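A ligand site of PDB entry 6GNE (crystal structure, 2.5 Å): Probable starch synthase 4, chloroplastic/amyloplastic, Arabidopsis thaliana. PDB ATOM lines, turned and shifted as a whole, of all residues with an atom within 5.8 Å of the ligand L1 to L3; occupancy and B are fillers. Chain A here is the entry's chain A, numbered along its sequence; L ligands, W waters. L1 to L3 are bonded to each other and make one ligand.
NE2 of Gln 321 sits at hydrogen-bond distance from O4 of LG3 L3, 2.9 Å away. O5 of LG3 L3 lies within hydrogen-bond range of OE1 of Glu 397, at 2.7 Å. The side-chain carboxylate of Asp 146 is in hydrogen-bond range of an oxygen (O1) of LG3 L3 (2.4 Å). An oxygen (O1) of LG4 L4 is in hydrogen-bond range of the backbone NH of Gly 27 (2.9 Å). The side-chain amide nitrogen (NE2) of Gln 148 is in hydrogen-bond range of an oxygen (O2) of LG2 L2, at 2.8 Å. NE1 of Trp 147 is in hydrogen-bond range of O1 of LG2 L2, at 3.1 Å. An oxygen (O5) of LG2 L2 lies within hydrogen-bond range of the guanidinium group (NH1) of Arg 317 (3.5 Å). The side-chain amide oxygen (OD1) of Asn 262 lies within hydrogen-bond range of an oxygen (O7) of LG3 L3 (2.7 Å). O3 of LG4 L4 is in salt-bridge range of NZ of Lys 322 (2.9 Å). A ring nitrogen (ND1) of His 175 lies within hydrogen-bond range of an oxygen (O7) of LG3 L3. An oxygen (O4) of LG4 L4 sits at hydrogen-bond distance from the backbone NH of Leu 401 (2.8 Å). NE of Arg 317 is in salt-bridge range of O2 of LG4 L4, 2.7 Å away. O5 of LG3 L3 is in hydrogen-bond range of N of Cys 399, 3.1 Å away. N of Gly 400 is in hydrogen-bond range of O6 of LG3 L3 (2.9 Å).
O3 of LG4 L4 lies within hydrogen-bond range of O4 of LG3 L3, 2.6 Å away.
The backbone NH (N) of Asn 262 lies within hydrogen-bond range of the backbone carbonyl oxygen (O) of Val 229 (3.2 Å). The backbone carbonyl oxygen (O) of Val 229 sits close to the side-chain sulfur (SG) of Cys 399. The backbone NH (N) of Gly 26 lies within hydrogen-bond range of the side-chain carboxylate (OE1) of Glu 18 (3.3 Å). The side-chain amide oxygen (OD1) of Asn 262 sits close to the side-chain sulfur (SG) of Cys 399 (3.6 Å). The side-chain amide oxygen of Gln 321 sits at hydrogen-bond distance from the side-chain amide nitrogen of Asn 176 (3.5 Å). The side-chain carboxylate of Glu 397 lies within salt-bridge range of the side-chain amino group of Lys 322, at 2.8 Å. The backbone NH (N) of His 175 is in hydrogen-bond range of the side-chain carboxylate (OD1) of Asp 146 (2.6 Å). NE2 of Gln 321 sits at hydrogen-bond distance from OE1 of Glu 397, at 3.1 Å.
Residues that only touch the ligand L1 to L3: Pro 398 (3.4 Å), Val 229 (3.4 Å), Asn 176 (3.5 Å), Gly 27 (3.5 Å), Tyr 179 (3.5 Å), Val 31 (3.6 Å), Leu 28 (3.7 Å), Tyr 112 (3.9 Å) and Gly 26 (3.9 Å). Hydrophobic or aromatic side chains that line the ligand L1 to L3: Val 31, Tyr 112, Trp 147, His 175, Tyr 179, Val 229 and Pro 398. 19 residues have an atom within 4 Å of the ligand L1 to L3: Gly 26, Gly 27, Leu 28, Val 31, Tyr 112, Asp 146, Trp 147, Gln 148, His 175, Asn 176, Tyr 179, Val 229, Asn 262, Arg 317, Gln 321, Glu 397, Pro 398, Cys 399 and Gly 400. The nearest printed residue that does not touch the ligand L1 to L3 is Glu 18 (4.02 Å).
Water W1 lies within hydrogen-bond range of O4 of LG3 L3 (2.9 Å), ND2 of Asn 176 (2.9 Å), OE1 of Gln 321 (3.0 Å) and NH2 of Arg 317 (3.1 Å). Water W3 lies within hydrogen-bond range of the side-chain carboxylate of Asp 117, an oxygen (O1) of LG2 L2 and the side-chain amide nitrogen of Gln 148.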
ATOM      1  N   GLU A  18     -12.556 -20.627  -4.075  1.00  0.00           N
ATOM      2  CA  GLU A  18     -11.451 -21.594  -4.140  1.00  0.00           C
ATOM      3  C   GLU A  18     -10.210 -21.054  -4.839  1.00  0.00           C
ATOM      4  O   GLU A  18     -10.289 -20.193  -5.733  1.00  0.00           O
ATOM      5  CB  GLU A  18     -11.855 -22.837  -4.938  1.00  0.00           C
ATOM      6  CG  GLU A  18     -12.958 -23.695  -4.365  1.00  0.00           C
ATOM      7  CD  GLU A  18     -13.325 -24.822  -5.334  1.00  0.00           C
ATOM      8  OE1 GLU A  18     -12.433 -25.644  -5.711  1.00  0.00           O
ATOM      9  OE2 GLU A  18     -14.506 -24.891  -5.732  1.00  0.00           O
ATOM     10  N   VAL A  25     -11.778 -27.819  -4.121  1.00  0.00           N
ATOM     11  CA  VAL A  25     -12.763 -28.899  -4.207  1.00  0.00           C
ATOM     12  C   VAL A  25     -12.702 -29.568  -5.586  1.00  0.00           C
ATOM     13  O   VAL A  25     -12.722 -30.786  -5.677  1.00  0.00           O
ATOM     14  CB  VAL A  25     -14.188 -28.369  -3.914  1.00  0.00           C
ATOM     15  CG1 VAL A  25     -15.248 -29.452  -4.214  1.00  0.00           C
ATOM     16  CG2 VAL A  25     -14.276 -27.897  -2.464  1.00  0.00           C
ATOM     17  N   GLY A  26     -12.701 -28.784  -6.651  1.00  0.00           N
ATOM     18  CA  GLY A  26     -12.450 -29.319  -7.971  1.00  0.00           C
ATOM     19  C   GLY A  26     -11.744 -28.362  -8.892  1.00  0.00           C
ATOM     20  O   GLY A  26     -10.771 -27.724  -8.522  1.00  0.00           O
ATOM     21  N   GLY A  27     -12.253 -28.256 -10.119  1.00  0.00           N
ATOM     22  CA  GLY A  27     -11.597 -27.516 -11.151  1.00  0.00           C
ATOM     23  C   GLY A  27     -11.583 -26.002 -10.997  1.00  0.00           C
ATOM     24  O   GLY A  27     -10.708 -25.344 -11.553  1.00  0.00           O
ATOM     25  N   LEU A  28     -12.565 -25.461 -10.284  1.00  0.00           N
ATOM     26  CA  LEU A  28     -12.666 -24.015 -10.082  1.00  0.00           C
ATOM     27  C   LEU A  28     -11.406 -23.505  -9.420  1.00  0.00           C
ATOM     28  O   LEU A  28     -10.741 -22.610  -9.909  1.00  0.00           O
ATOM     29  CB  LEU A  28     -13.891 -23.644  -9.244  1.00  0.00           C
ATOM     30  CG  LEU A  28     -14.148 -22.118  -9.241  1.00  0.00           C
ATOM     31  CD1 LEU A  28     -15.633 -21.788  -9.415  1.00  0.00           C
ATOM     32  CD2 LEU A  28     -13.631 -21.525  -7.954  1.00  0.00           C
ATOM     33  N   VAL A  31      -8.456 -23.504 -11.786  1.00  0.00           N
ATOM     34  CA  VAL A  31      -8.549 -22.433 -12.753  1.00  0.00           C
ATOM     35  C   VAL A  31      -8.141 -21.086 -12.180  1.00  0.00           C
ATOM     36  O   VAL A  31      -7.408 -20.320 -12.825  1.00  0.00           O
ATOM     37  CB  VAL A  31      -9.958 -22.383 -13.389  1.00  0.00           C
ATOM     38  CG1 VAL A  31     -10.162 -21.116 -14.234  1.00  0.00           C
ATOM     39  CG2 VAL A  31     -10.168 -23.663 -14.238  1.00  0.00           C
ATOM     40  N   TYR A 112     -17.964 -26.307   1.030  1.00  0.00           N
ATOM     41  CA  TYR A 112     -19.343 -26.144   0.557  1.00  0.00           C
ATOM     42  C   TYR A 112     -20.260 -27.108   1.273  1.00  0.00           C
ATOM     43  O   TYR A 112     -19.816 -28.036   1.915  1.00  0.00           O
ATOM     44  CB  TYR A 112     -19.454 -26.450  -0.923  1.00  0.00           C
ATOM     45  CG  TYR A 112     -18.562 -25.665  -1.844  1.00  0.00           C
ATOM     46  CD1 TYR A 112     -18.468 -24.282  -1.737  1.00  0.00           C
ATOM     47  CD2 TYR A 112     -17.872 -26.296  -2.877  1.00  0.00           C
ATOM     48  CE1 TYR A 112     -17.690 -23.555  -2.610  1.00  0.00           C
ATOM     49  CE2 TYR A 112     -17.067 -25.592  -3.749  1.00  0.00           C
ATOM     50  CZ  TYR A 112     -16.967 -24.201  -3.620  1.00  0.00           C
ATOM     51  OH  TYR A 112     -16.196 -23.474  -4.500  1.00  0.00           O
ATOM     52  N   GLY A 113     -21.561 -26.845   1.145  1.00  0.00           N
ATOM     53  CA  GLY A 113     -22.597 -27.769   1.548  1.00  0.00           C
ATOM     54  C   GLY A 113     -23.298 -27.487   2.852  1.00  0.00           C
ATOM     55  O   GLY A 113     -24.043 -28.326   3.325  1.00  0.00           O
ATOM     56  N   ASP A 117     -25.372 -21.728   2.914  1.00  0.00           N
ATOM     57  CA  ASP A 117     -24.330 -21.328   1.927  1.00  0.00           C
ATOM     58  C   ASP A 117     -24.582 -19.933   1.340  1.00  0.00           C
ATOM     59  O   ASP A 117     -23.638 -19.166   1.150  1.00  0.00           O
ATOM     60  CB  ASP A 117     -24.190 -22.346   0.772  1.00  0.00           C
ATOM     61  CG  ASP A 117     -23.230 -23.495   1.090  1.00  0.00           C
ATOM     62  OD1 ASP A 117     -22.556 -23.501   2.127  1.00  0.00           O
ATOM     63  OD2 ASP A 117     -23.129 -24.392   0.249  1.00  0.00           O
ATOM     64  N   ASP A 146     -18.480 -18.006 -10.334  1.00  0.00           N
ATOM     65  CA  ASP A 146     -19.626 -18.864  -9.935  1.00  0.00           C
ATOM     66  C   ASP A 146     -20.590 -18.187  -8.980  1.00  0.00           C
ATOM     67  O   ASP A 146     -20.397 -17.027  -8.622  1.00  0.00           O
ATOM     68  CB  ASP A 146     -19.144 -20.252  -9.448  1.00  0.00           C
ATOM     69  CG  ASP A 146     -18.956 -21.247 -10.561  1.00  0.00           C
ATOM     70  OD1 ASP A 146     -18.711 -20.805 -11.688  1.00  0.00           O
ATOM     71  OD2 ASP A 146     -19.100 -22.467 -10.364  1.00  0.00           O
ATOM     72  N   TRP A 147     -21.654 -18.898  -8.588  1.00  0.00           N
ATOM     73  CA  TRP A 147     -22.738 -18.262  -7.854  1.00  0.00           C
ATOM     74  C   TRP A 147     -22.273 -17.660  -6.534  1.00  0.00           C
ATOM     75  O   TRP A 147     -22.781 -16.611  -6.144  1.00  0.00           O
ATOM     76  CB  TRP A 147     -23.936 -19.214  -7.676  1.00  0.00           C
ATOM     77  CG  TRP A 147     -23.776 -20.230  -6.597  1.00  0.00           C
ATOM     78  CD1 TRP A 147     -23.349 -21.511  -6.732  1.00  0.00           C
ATOM     79  CD2 TRP A 147     -24.058 -20.053  -5.200  1.00  0.00           C
ATOM     80  NE1 TRP A 147     -23.338 -22.130  -5.507  1.00  0.00           N
ATOM     81  CE2 TRP A 147     -23.762 -21.255  -4.555  1.00  0.00           C
ATOM     82  CE3 TRP A 147     -24.531 -18.974  -4.440  1.00  0.00           C
ATOM     83  CZ2 TRP A 147     -23.932 -21.436  -3.176  1.00  0.00           C
ATOM     84  CZ3 TRP A 147     -24.699 -19.134  -3.073  1.00  0.00           C
ATOM     85  CH2 TRP A 147     -24.409 -20.363  -2.452  1.00  0.00           C
ATOM     86  N   GLN A 148     -21.304 -18.289  -5.880  1.00  0.00           N
ATOM     87  CA  GLN A 148     -20.847 -17.815  -4.573  1.00  0.00           C
ATOM     88  C   GLN A 148     -20.334 -16.357  -4.572  1.00  0.00           C
ATOM     89  O   GLN A 148     -20.568 -15.604  -3.614  1.00  0.00           O
ATOM     90  CB  GLN A 148     -19.772 -18.745  -4.003  1.00  0.00           C
ATOM     91  CG  GLN A 148     -20.271 -20.125  -3.596  1.00  0.00           C
ATOM     92  CD  GLN A 148     -20.213 -21.162  -4.725  1.00  0.00           C
ATOM     93  OE1 GLN A 148     -20.126 -20.805  -5.902  1.00  0.00           O
ATOM     94  NE2 GLN A 148     -20.248 -22.455  -4.368  1.00  0.00           N
ATOM     95  N   HIS A 175     -18.466 -21.484 -14.156  1.00  0.00           N
ATOM     96  CA  HIS A 175     -17.771 -22.758 -14.423  1.00  0.00           C
ATOM     97  C   HIS A 175     -18.755 -23.973 -14.465  1.00  0.00           C
ATOM     98  O   HIS A 175     -18.365 -25.093 -14.873  1.00  0.00           O
ATOM     99  CB  HIS A 175     -16.743 -23.023 -13.329  1.00  0.00           C
ATOM    100  CG  HIS A 175     -15.656 -22.002 -13.232  1.00  0.00           C
ATOM    101  ND1 HIS A 175     -14.349 -22.292 -13.534  1.00  0.00           N
ATOM    102  CD2 HIS A 175     -15.670 -20.728 -12.775  1.00  0.00           C
ATOM    103  CE1 HIS A 175     -13.610 -21.221 -13.321  1.00  0.00           C
ATOM    104  NE2 HIS A 175     -14.385 -20.264 -12.864  1.00  0.00           N
ATOM    105  N   ASN A 176     -19.981 -23.764 -14.006  1.00  0.00           N
ATOM    106  CA  ASN A 176     -21.066 -24.738 -14.177  1.00  0.00           C
ATOM    107  C   ASN A 176     -22.411 -24.074 -13.956  1.00  0.00           C
ATOM    108  O   ASN A 176     -22.760 -23.746 -12.822  1.00  0.00           O
ATOM    109  CB  ASN A 176     -20.889 -25.945 -13.208  1.00  0.00           C
ATOM    110  CG  ASN A 176     -21.916 -27.059 -13.422  1.00  0.00           C
ATOM    111  OD1 ASN A 176     -22.806 -26.931 -14.246  1.00  0.00           O
ATOM    112  ND2 ASN A 176     -21.798 -28.140 -12.674  1.00  0.00           N
ATOM    113  N   TYR A 179     -25.217 -24.689 -11.187  1.00  0.00           N
ATOM    114  CA  TYR A 179     -25.230 -24.080  -9.846  1.00  0.00           C
ATOM    115  C   TYR A 179     -25.477 -22.598  -9.911  1.00  0.00           C
ATOM    116  O   TYR A 179     -24.558 -21.835 -10.146  1.00  0.00           O
ATOM    117  CB  TYR A 179     -23.944 -24.417  -9.085  1.00  0.00           C
ATOM    118  CG  TYR A 179     -23.755 -25.915  -8.934  1.00  0.00           C
ATOM    119  CD1 TYR A 179     -24.812 -26.734  -8.460  1.00  0.00           C
ATOM    120  CD2 TYR A 179     -22.512 -26.523  -9.244  1.00  0.00           C
ATOM    121  CE1 TYR A 179     -24.647 -28.115  -8.350  1.00  0.00           C
ATOM    122  CE2 TYR A 179     -22.329 -27.917  -9.113  1.00  0.00           C
ATOM    123  CZ  TYR A 179     -23.387 -28.703  -8.671  1.00  0.00           C
ATOM    124  OH  TYR A 179     -23.236 -30.036  -8.529  1.00  0.00           O
ATOM    125  N   VAL A 229     -16.384 -21.913 -19.594  1.00  0.00           N
ATOM    126  CA  VAL A 229     -15.099 -22.582 -19.621  1.00  0.00           C
ATOM    127  C   VAL A 229     -14.817 -23.491 -20.853  1.00  0.00           C
ATOM    128  O   VAL A 229     -13.753 -24.177 -20.881  1.00  0.00           O
ATOM    129  CB  VAL A 229     -14.870 -23.288 -18.264  1.00  0.00           C
ATOM    130  CG1 VAL A 229     -14.730 -22.219 -17.178  1.00  0.00           C
ATOM    131  CG2 VAL A 229     -16.030 -24.238 -17.932  1.00  0.00           C
ATOM    132  N   ASN A 262     -10.566 -23.746 -20.694  1.00  0.00           N
ATOM    133  CA  ASN A 262      -9.556 -23.694 -19.628  1.00  0.00           C
ATOM    134  C   ASN A 262      -8.220 -24.309 -20.123  1.00  0.00           C
ATOM    135  O   ASN A 262      -8.213 -25.266 -20.921  1.00  0.00           O
ATOM    136  CB  ASN A 262      -9.999 -24.497 -18.404  1.00  0.00           C
ATOM    137  CG  ASN A 262     -11.186 -23.916 -17.671  1.00  0.00           C
ATOM    138  OD1 ASN A 262     -11.900 -24.667 -16.988  1.00  0.00           O
ATOM    139  ND2 ASN A 262     -11.366 -22.599 -17.738  1.00  0.00           N
ATOM    140  N   ARG A 317     -14.924 -36.622  -8.942  1.00  0.00           N
ATOM    141  CA  ARG A 317     -15.971 -36.579  -7.948  1.00  0.00           C
ATOM    142  C   ARG A 317     -17.040 -37.494  -8.518  1.00  0.00           C
ATOM    143  O   ARG A 317     -17.263 -37.520  -9.704  1.00  0.00           O
ATOM    144  CB  ARG A 317     -16.507 -35.137  -7.751  1.00  0.00           C
ATOM    145  CG  ARG A 317     -15.451 -34.184  -7.164  1.00  0.00           C
ATOM    146  CD  ARG A 317     -15.814 -32.688  -7.195  1.00  0.00           C
ATOM    147  NE  ARG A 317     -16.397 -32.289  -8.486  1.00  0.00           N
ATOM    148  CZ  ARG A 317     -17.703 -32.163  -8.748  1.00  0.00           C
ATOM    149  NH1 ARG A 317     -18.589 -32.398  -7.788  1.00  0.00           N
ATOM    150  NH2 ARG A 317     -18.137 -31.790  -9.971  1.00  0.00           N
ATOM    151  N   VAL A 319     -20.500 -37.889  -8.890  1.00  0.00           N
ATOM    152  CA  VAL A 319     -21.815 -37.220  -8.944  1.00  0.00           C
ATOM    153  C   VAL A 319     -22.415 -37.486 -10.322  1.00  0.00           C
ATOM    154  O   VAL A 319     -21.694 -37.756 -11.260  1.00  0.00           O
ATOM    155  CB  VAL A 319     -21.667 -35.685  -8.676  1.00  0.00           C
ATOM    156  CG1 VAL A 319     -21.062 -35.450  -7.293  1.00  0.00           C
ATOM    157  CG2 VAL A 319     -20.784 -34.978  -9.719  1.00  0.00           C
ATOM    158  N   GLN A 321     -23.200 -35.860 -12.861  1.00  0.00           N
ATOM    159  CA  GLN A 321     -22.582 -35.178 -13.987  1.00  0.00           C
ATOM    160  C   GLN A 321     -21.510 -36.039 -14.680  1.00  0.00           C
ATOM    161  O   GLN A 321     -21.375 -36.020 -15.935  1.00  0.00           O
ATOM    162  CB  GLN A 321     -21.975 -33.863 -13.520  1.00  0.00           C
ATOM    163  CG  GLN A 321     -21.145 -33.112 -14.564  1.00  0.00           C
ATOM    164  CD  GLN A 321     -20.339 -31.971 -13.989  1.00  0.00           C
ATOM    165  OE1 GLN A 321     -20.720 -31.408 -12.963  1.00  0.00           O
ATOM    166  NE2 GLN A 321     -19.215 -31.630 -14.646  1.00  0.00           N
ATOM    167  N   LYS A 322     -20.769 -36.782 -13.864  1.00  0.00           N
ATOM    168  CA  LYS A 322     -19.600 -37.520 -14.330  1.00  0.00           C
ATOM    169  C   LYS A 322     -19.921 -38.897 -14.955  1.00  0.00           C
ATOM    170  O   LYS A 322     -19.001 -39.629 -15.342  1.00  0.00           O
ATOM    171  CB  LYS A 322     -18.645 -37.699 -13.148  1.00  0.00           C
ATOM    172  CG  LYS A 322     -18.206 -36.378 -12.539  1.00  0.00           C
ATOM    173  CD  LYS A 322     -17.362 -35.536 -13.501  1.00  0.00           C
ATOM    174  CE  LYS A 322     -16.755 -34.345 -12.803  1.00  0.00           C
ATOM    175  NZ  LYS A 322     -16.202 -33.347 -13.734  1.00  0.00           N
ATOM    176  N   PRO A 348     -20.346 -36.800  -2.587  1.00  0.00           N
ATOM    177  CA  PRO A 348     -21.142 -36.206  -1.510  1.00  0.00           C
ATOM    178  C   PRO A 348     -22.535 -36.841  -1.369  1.00  0.00           C
ATOM    179  O   PRO A 348     -23.248 -36.460  -0.434  1.00  0.00           O
ATOM    180  CB  PRO A 348     -21.300 -34.749  -1.983  1.00  0.00           C
ATOM    181  CG  PRO A 348     -21.324 -34.837  -3.477  1.00  0.00           C
ATOM    182  CD  PRO A 348     -20.437 -36.022  -3.840  1.00  0.00           C
ATOM    183  N   GLU A 397     -20.201 -31.705 -19.250  1.00  0.00           N
ATOM    184  CA  GLU A 397     -18.906 -31.311 -18.753  1.00  0.00           C
ATOM    185  C   GLU A 397     -18.544 -29.908 -19.291  1.00  0.00           C
ATOM    186  O   GLU A 397     -18.090 -29.760 -20.427  1.00  0.00           O
ATOM    187  CB  GLU A 397     -17.859 -32.363 -19.138  1.00  0.00           C
ATOM    188  CG  GLU A 397     -16.559 -32.269 -18.363  1.00  0.00           C
ATOM    189  CD  GLU A 397     -16.714 -32.631 -16.892  1.00  0.00           C
ATOM    190  OE1 GLU A 397     -16.509 -31.751 -16.062  1.00  0.00           O
ATOM    191  OE2 GLU A 397     -17.028 -33.774 -16.553  1.00  0.00           O
ATOM    192  N   PRO A 398     -18.761 -28.862 -18.461  1.00  0.00           N
ATOM    193  CA  PRO A 398     -18.452 -27.495 -18.815  1.00  0.00           C
ATOM    194  C   PRO A 398     -17.073 -27.326 -19.423  1.00  0.00           C
ATOM    195  O   PRO A 398     -16.928 -26.677 -20.446  1.00  0.00           O
ATOM    196  CB  PRO A 398     -18.535 -26.771 -17.476  1.00  0.00           C
ATOM    197  CG  PRO A 398     -19.603 -27.518 -16.717  1.00  0.00           C
ATOM    198  CD  PRO A 398     -19.425 -28.947 -17.138  1.00  0.00           C
ATOM    199  N   CYS A 399     -16.080 -27.935 -18.786  1.00  0.00           N
ATOM    200  CA  CYS A 399     -14.759 -28.056 -19.377  1.00  0.00           C
ATOM    201  C   CYS A 399     -14.131 -29.412 -19.088  1.00  0.00           C
ATOM    202  O   CYS A 399     -13.911 -30.219 -20.002  1.00  0.00           O
ATOM    203  CB  CYS A 399     -13.838 -26.949 -18.930  1.00  0.00           C
ATOM    204  SG  CYS A 399     -12.212 -27.036 -19.734  1.00  0.00           S
ATOM    205  N   GLY A 400     -13.819 -29.660 -17.835  1.00  0.00           N
ATOM    206  CA  GLY A 400     -13.034 -30.805 -17.447  1.00  0.00           C
ATOM    207  C   GLY A 400     -11.542 -30.515 -17.619  1.00  0.00           C
ATOM    208  O   GLY A 400     -11.100 -30.023 -18.666  1.00  0.00           O
ATOM    209  N   LEU A 401     -10.788 -30.799 -16.573  1.00  0.00           N
ATOM    210  CA  LEU A 401      -9.357 -30.637 -16.543  1.00  0.00           C
ATOM    211  C   LEU A 401      -8.620 -31.974 -16.512  1.00  0.00           C
ATOM    212  O   LEU A 401      -7.459 -32.079 -16.967  1.00  0.00           O
ATOM    213  CB  LEU A 401      -8.976 -29.829 -15.317  1.00  0.00           C
ATOM    214  CG  LEU A 401      -9.619 -28.455 -15.172  1.00  0.00           C
ATOM    215  CD1 LEU A 401      -9.048 -27.770 -13.941  1.00  0.00           C
ATOM    216  CD2 LEU A 401      -9.400 -27.589 -16.395  1.00  0.00           C
HETATM  217  C1  LIG L   1     -27.135 -28.846  -3.944  1.00  0.00           C
HETATM  218  C2  LIG L   1     -26.769 -27.381  -3.620  1.00  0.00           C
HETATM  219  C3  LIG L   1     -25.503 -26.940  -4.355  1.00  0.00           C
HETATM  220  C4  LIG L   1     -24.364 -27.913  -3.989  1.00  0.00           C
HETATM  221  C5  LIG L   1     -24.788 -29.340  -4.351  1.00  0.00           C
HETATM  222  C6  LIG L   1     -23.699 -30.376  -4.032  1.00  0.00           C
HETATM  223  O1  LIG L   1     -27.518 -28.954  -5.323  1.00  0.00           O
HETATM  224  O2  LIG L   1     -27.844 -26.521  -4.005  1.00  0.00           O
HETATM  225  O3  LIG L   1     -25.181 -25.557  -4.085  1.00  0.00           O
HETATM  226  O4  LIG L   1     -23.196 -27.565  -4.735  1.00  0.00           O
HETATM  227  O5  LIG L   1     -26.008 -29.698  -3.668  1.00  0.00           O
HETATM  228  O6  LIG L   1     -23.428 -30.313  -2.632  1.00  0.00           O
HETATM  229  C1  LG2 L   2     -22.026 -27.193  -4.044  1.00  0.00           C
HETATM  230  C2  LG2 L   2     -21.590 -25.781  -4.432  1.00  0.00           C
HETATM  231  C3  LG2 L   2     -21.145 -25.749  -5.894  1.00  0.00           C
HETATM  232  C4  LG2 L   2     -20.004 -26.737  -6.072  1.00  0.00           C
HETATM  233  C5  LG2 L   2     -20.501 -28.123  -5.708  1.00  0.00           C
HETATM  234  C6  LG2 L   2     -19.369 -29.141  -5.790  1.00  0.00           C
HETATM  235  O1  LG2 L   2     -22.644 -24.867  -4.168  1.00  0.00           O
HETATM  236  O2  LG2 L   2     -20.711 -24.448  -6.271  1.00  0.00           O
HETATM  237  O3  LG2 L   2     -19.512 -26.691  -7.414  1.00  0.00           O
HETATM  238  O4  LG2 L   2     -21.005 -28.129  -4.363  1.00  0.00           O
HETATM  239  O5  LG2 L   2     -19.815 -30.388  -5.237  1.00  0.00           O
HETATM  240  C1  LG3 L   3     -18.239 -26.067  -7.574  1.00  0.00           C
HETATM  241  O1  LG3 L   3     -19.310 -24.215  -8.704  1.00  0.00           O
HETATM  242  C2  LG3 L   3     -18.237 -25.166  -8.806  1.00  0.00           C
HETATM  243  C3  LG3 L   3     -14.983 -27.314 -15.061  1.00  0.00           C
HETATM  244  C4  LG3 L   3     -18.291 -25.976 -10.109  1.00  0.00           C
HETATM  245  O2  LG3 L   3     -18.221 -25.054 -11.198  1.00  0.00           O
HETATM  246  C5  LG3 L   3     -17.143 -27.000 -10.140  1.00  0.00           C
HETATM  247  N1  LG3 L   3     -17.052 -27.785 -11.377  1.00  0.00           N
HETATM  248  C6  LG3 L   3     -17.336 -27.880  -8.901  1.00  0.00           C
HETATM  249  O3  LG3 L   3     -17.229 -27.070  -7.722  1.00  0.00           O
HETATM  250  C7  LG3 L   3     -16.271 -28.947  -8.751  1.00  0.00           C
HETATM  251  C8  LG3 L   3     -16.802 -27.221 -12.712  1.00  0.00           C
HETATM  252  C9  LG3 L   3     -17.050 -28.205 -13.878  1.00  0.00           C
HETATM  253  O4  LG3 L   3     -17.701 -29.425 -13.477  1.00  0.00           O
HETATM  254  C10 LG3 L   3     -15.804 -28.551 -14.690  1.00  0.00           C
HETATM  255  O5  LG3 L   3     -16.265 -29.091 -15.925  1.00  0.00           O
HETATM  256  O6  LG3 L   3     -13.797 -27.731 -15.728  1.00  0.00           O
HETATM  257  C11 LG3 L   3     -14.684 -26.479 -13.855  1.00  0.00           C
HETATM  258  C12 LG3 L   3     -15.471 -26.489 -12.785  1.00  0.00           C
HETATM  259  C13 LG3 L   3     -13.487 -25.552 -13.878  1.00  0.00           C
HETATM  260  O7  LG3 L   3     -13.646 -24.553 -14.894  1.00  0.00           O
HETATM  261  P1  LG4 L   4     -14.859 -30.832 -11.544  1.00  0.00           P
HETATM  262  O1  LG4 L   4     -14.569 -29.354 -11.497  1.00  0.00           O
HETATM  263  O2  LG4 L   4     -14.490 -31.633 -10.333  1.00  0.00           O
HETATM  264  O3  LG4 L   4     -16.292 -31.075 -11.968  1.00  0.00           O
HETATM  265  P2  LG4 L   4     -12.570 -30.822 -13.313  1.00  0.00           P
HETATM  266  O4  LG4 L   4     -12.036 -31.855 -14.263  1.00  0.00           O
HETATM  267  O5  LG4 L   4     -12.774 -29.450 -13.905  1.00  0.00           O
HETATM  268  O6  LG4 L   4     -13.936 -31.444 -12.718  1.00  0.00           O
HETATM  269  O7  LG4 L   4     -11.612 -30.647 -12.039  1.00  0.00           O
HETATM  270  C1  LG4 L   4     -11.261 -31.743 -11.186  1.00  0.00           C
HETATM  271  C2  LG4 L   4      -9.970 -31.522 -10.371  1.00  0.00           C
HETATM  272  O8  LG4 L   4     -10.100 -32.149  -9.081  1.00  0.00           O
HETATM  273  C3  LG4 L   4      -8.763 -32.197 -10.990  1.00  0.00           C
HETATM  274  O9  LG4 L   4      -7.598 -31.496 -10.561  1.00  0.00           O
HETATM  275  C4  LG4 L   4      -8.754 -33.570 -10.366  1.00  0.00           C
HETATM  276  O10 LG4 L   4      -7.479 -34.171 -10.373  1.00  0.00           O
HETATM  277  C5  LG4 L   4      -9.196 -33.242  -8.969  1.00  0.00           C
HETATM  278  N1  LG4 L   4      -9.913 -34.355  -8.300  1.00  0.00           N
HETATM  279  C6  LG4 L   4     -11.176 -34.733  -8.479  1.00  0.00           C
HETATM  280  N2  LG4 L   4     -11.493 -35.754  -7.657  1.00  0.00           N
HETATM  281  C7  LG4 L   4     -10.409 -36.047  -6.917  1.00  0.00           C
HETATM  282  C8  LG4 L   4     -10.039 -37.024  -5.851  1.00  0.00           C
HETATM  283  N3  LG4 L   4     -10.950 -37.930  -5.407  1.00  0.00           N
HETATM  284  N4  LG4 L   4      -8.775 -36.960  -5.353  1.00  0.00           N
HETATM  285  C9  LG4 L   4      -7.870 -36.061  -5.819  1.00  0.00           C
HETATM  286  N5  LG4 L   4      -8.147 -35.171  -6.778  1.00  0.00           N
HETATM  287  C10 LG4 L   4      -9.368 -35.118  -7.361  1.00  0.00           C
HETATM  288  O   HOH W   1     -19.521 -29.281 -11.238  1.00  0.00           O
HETATM  289  O   HOH W   2     -14.011 -26.523  -7.992  1.00  0.00           O
HETATM  290  O   HOH W   3     -21.563 -23.535  -1.781  1.00  0.00           O
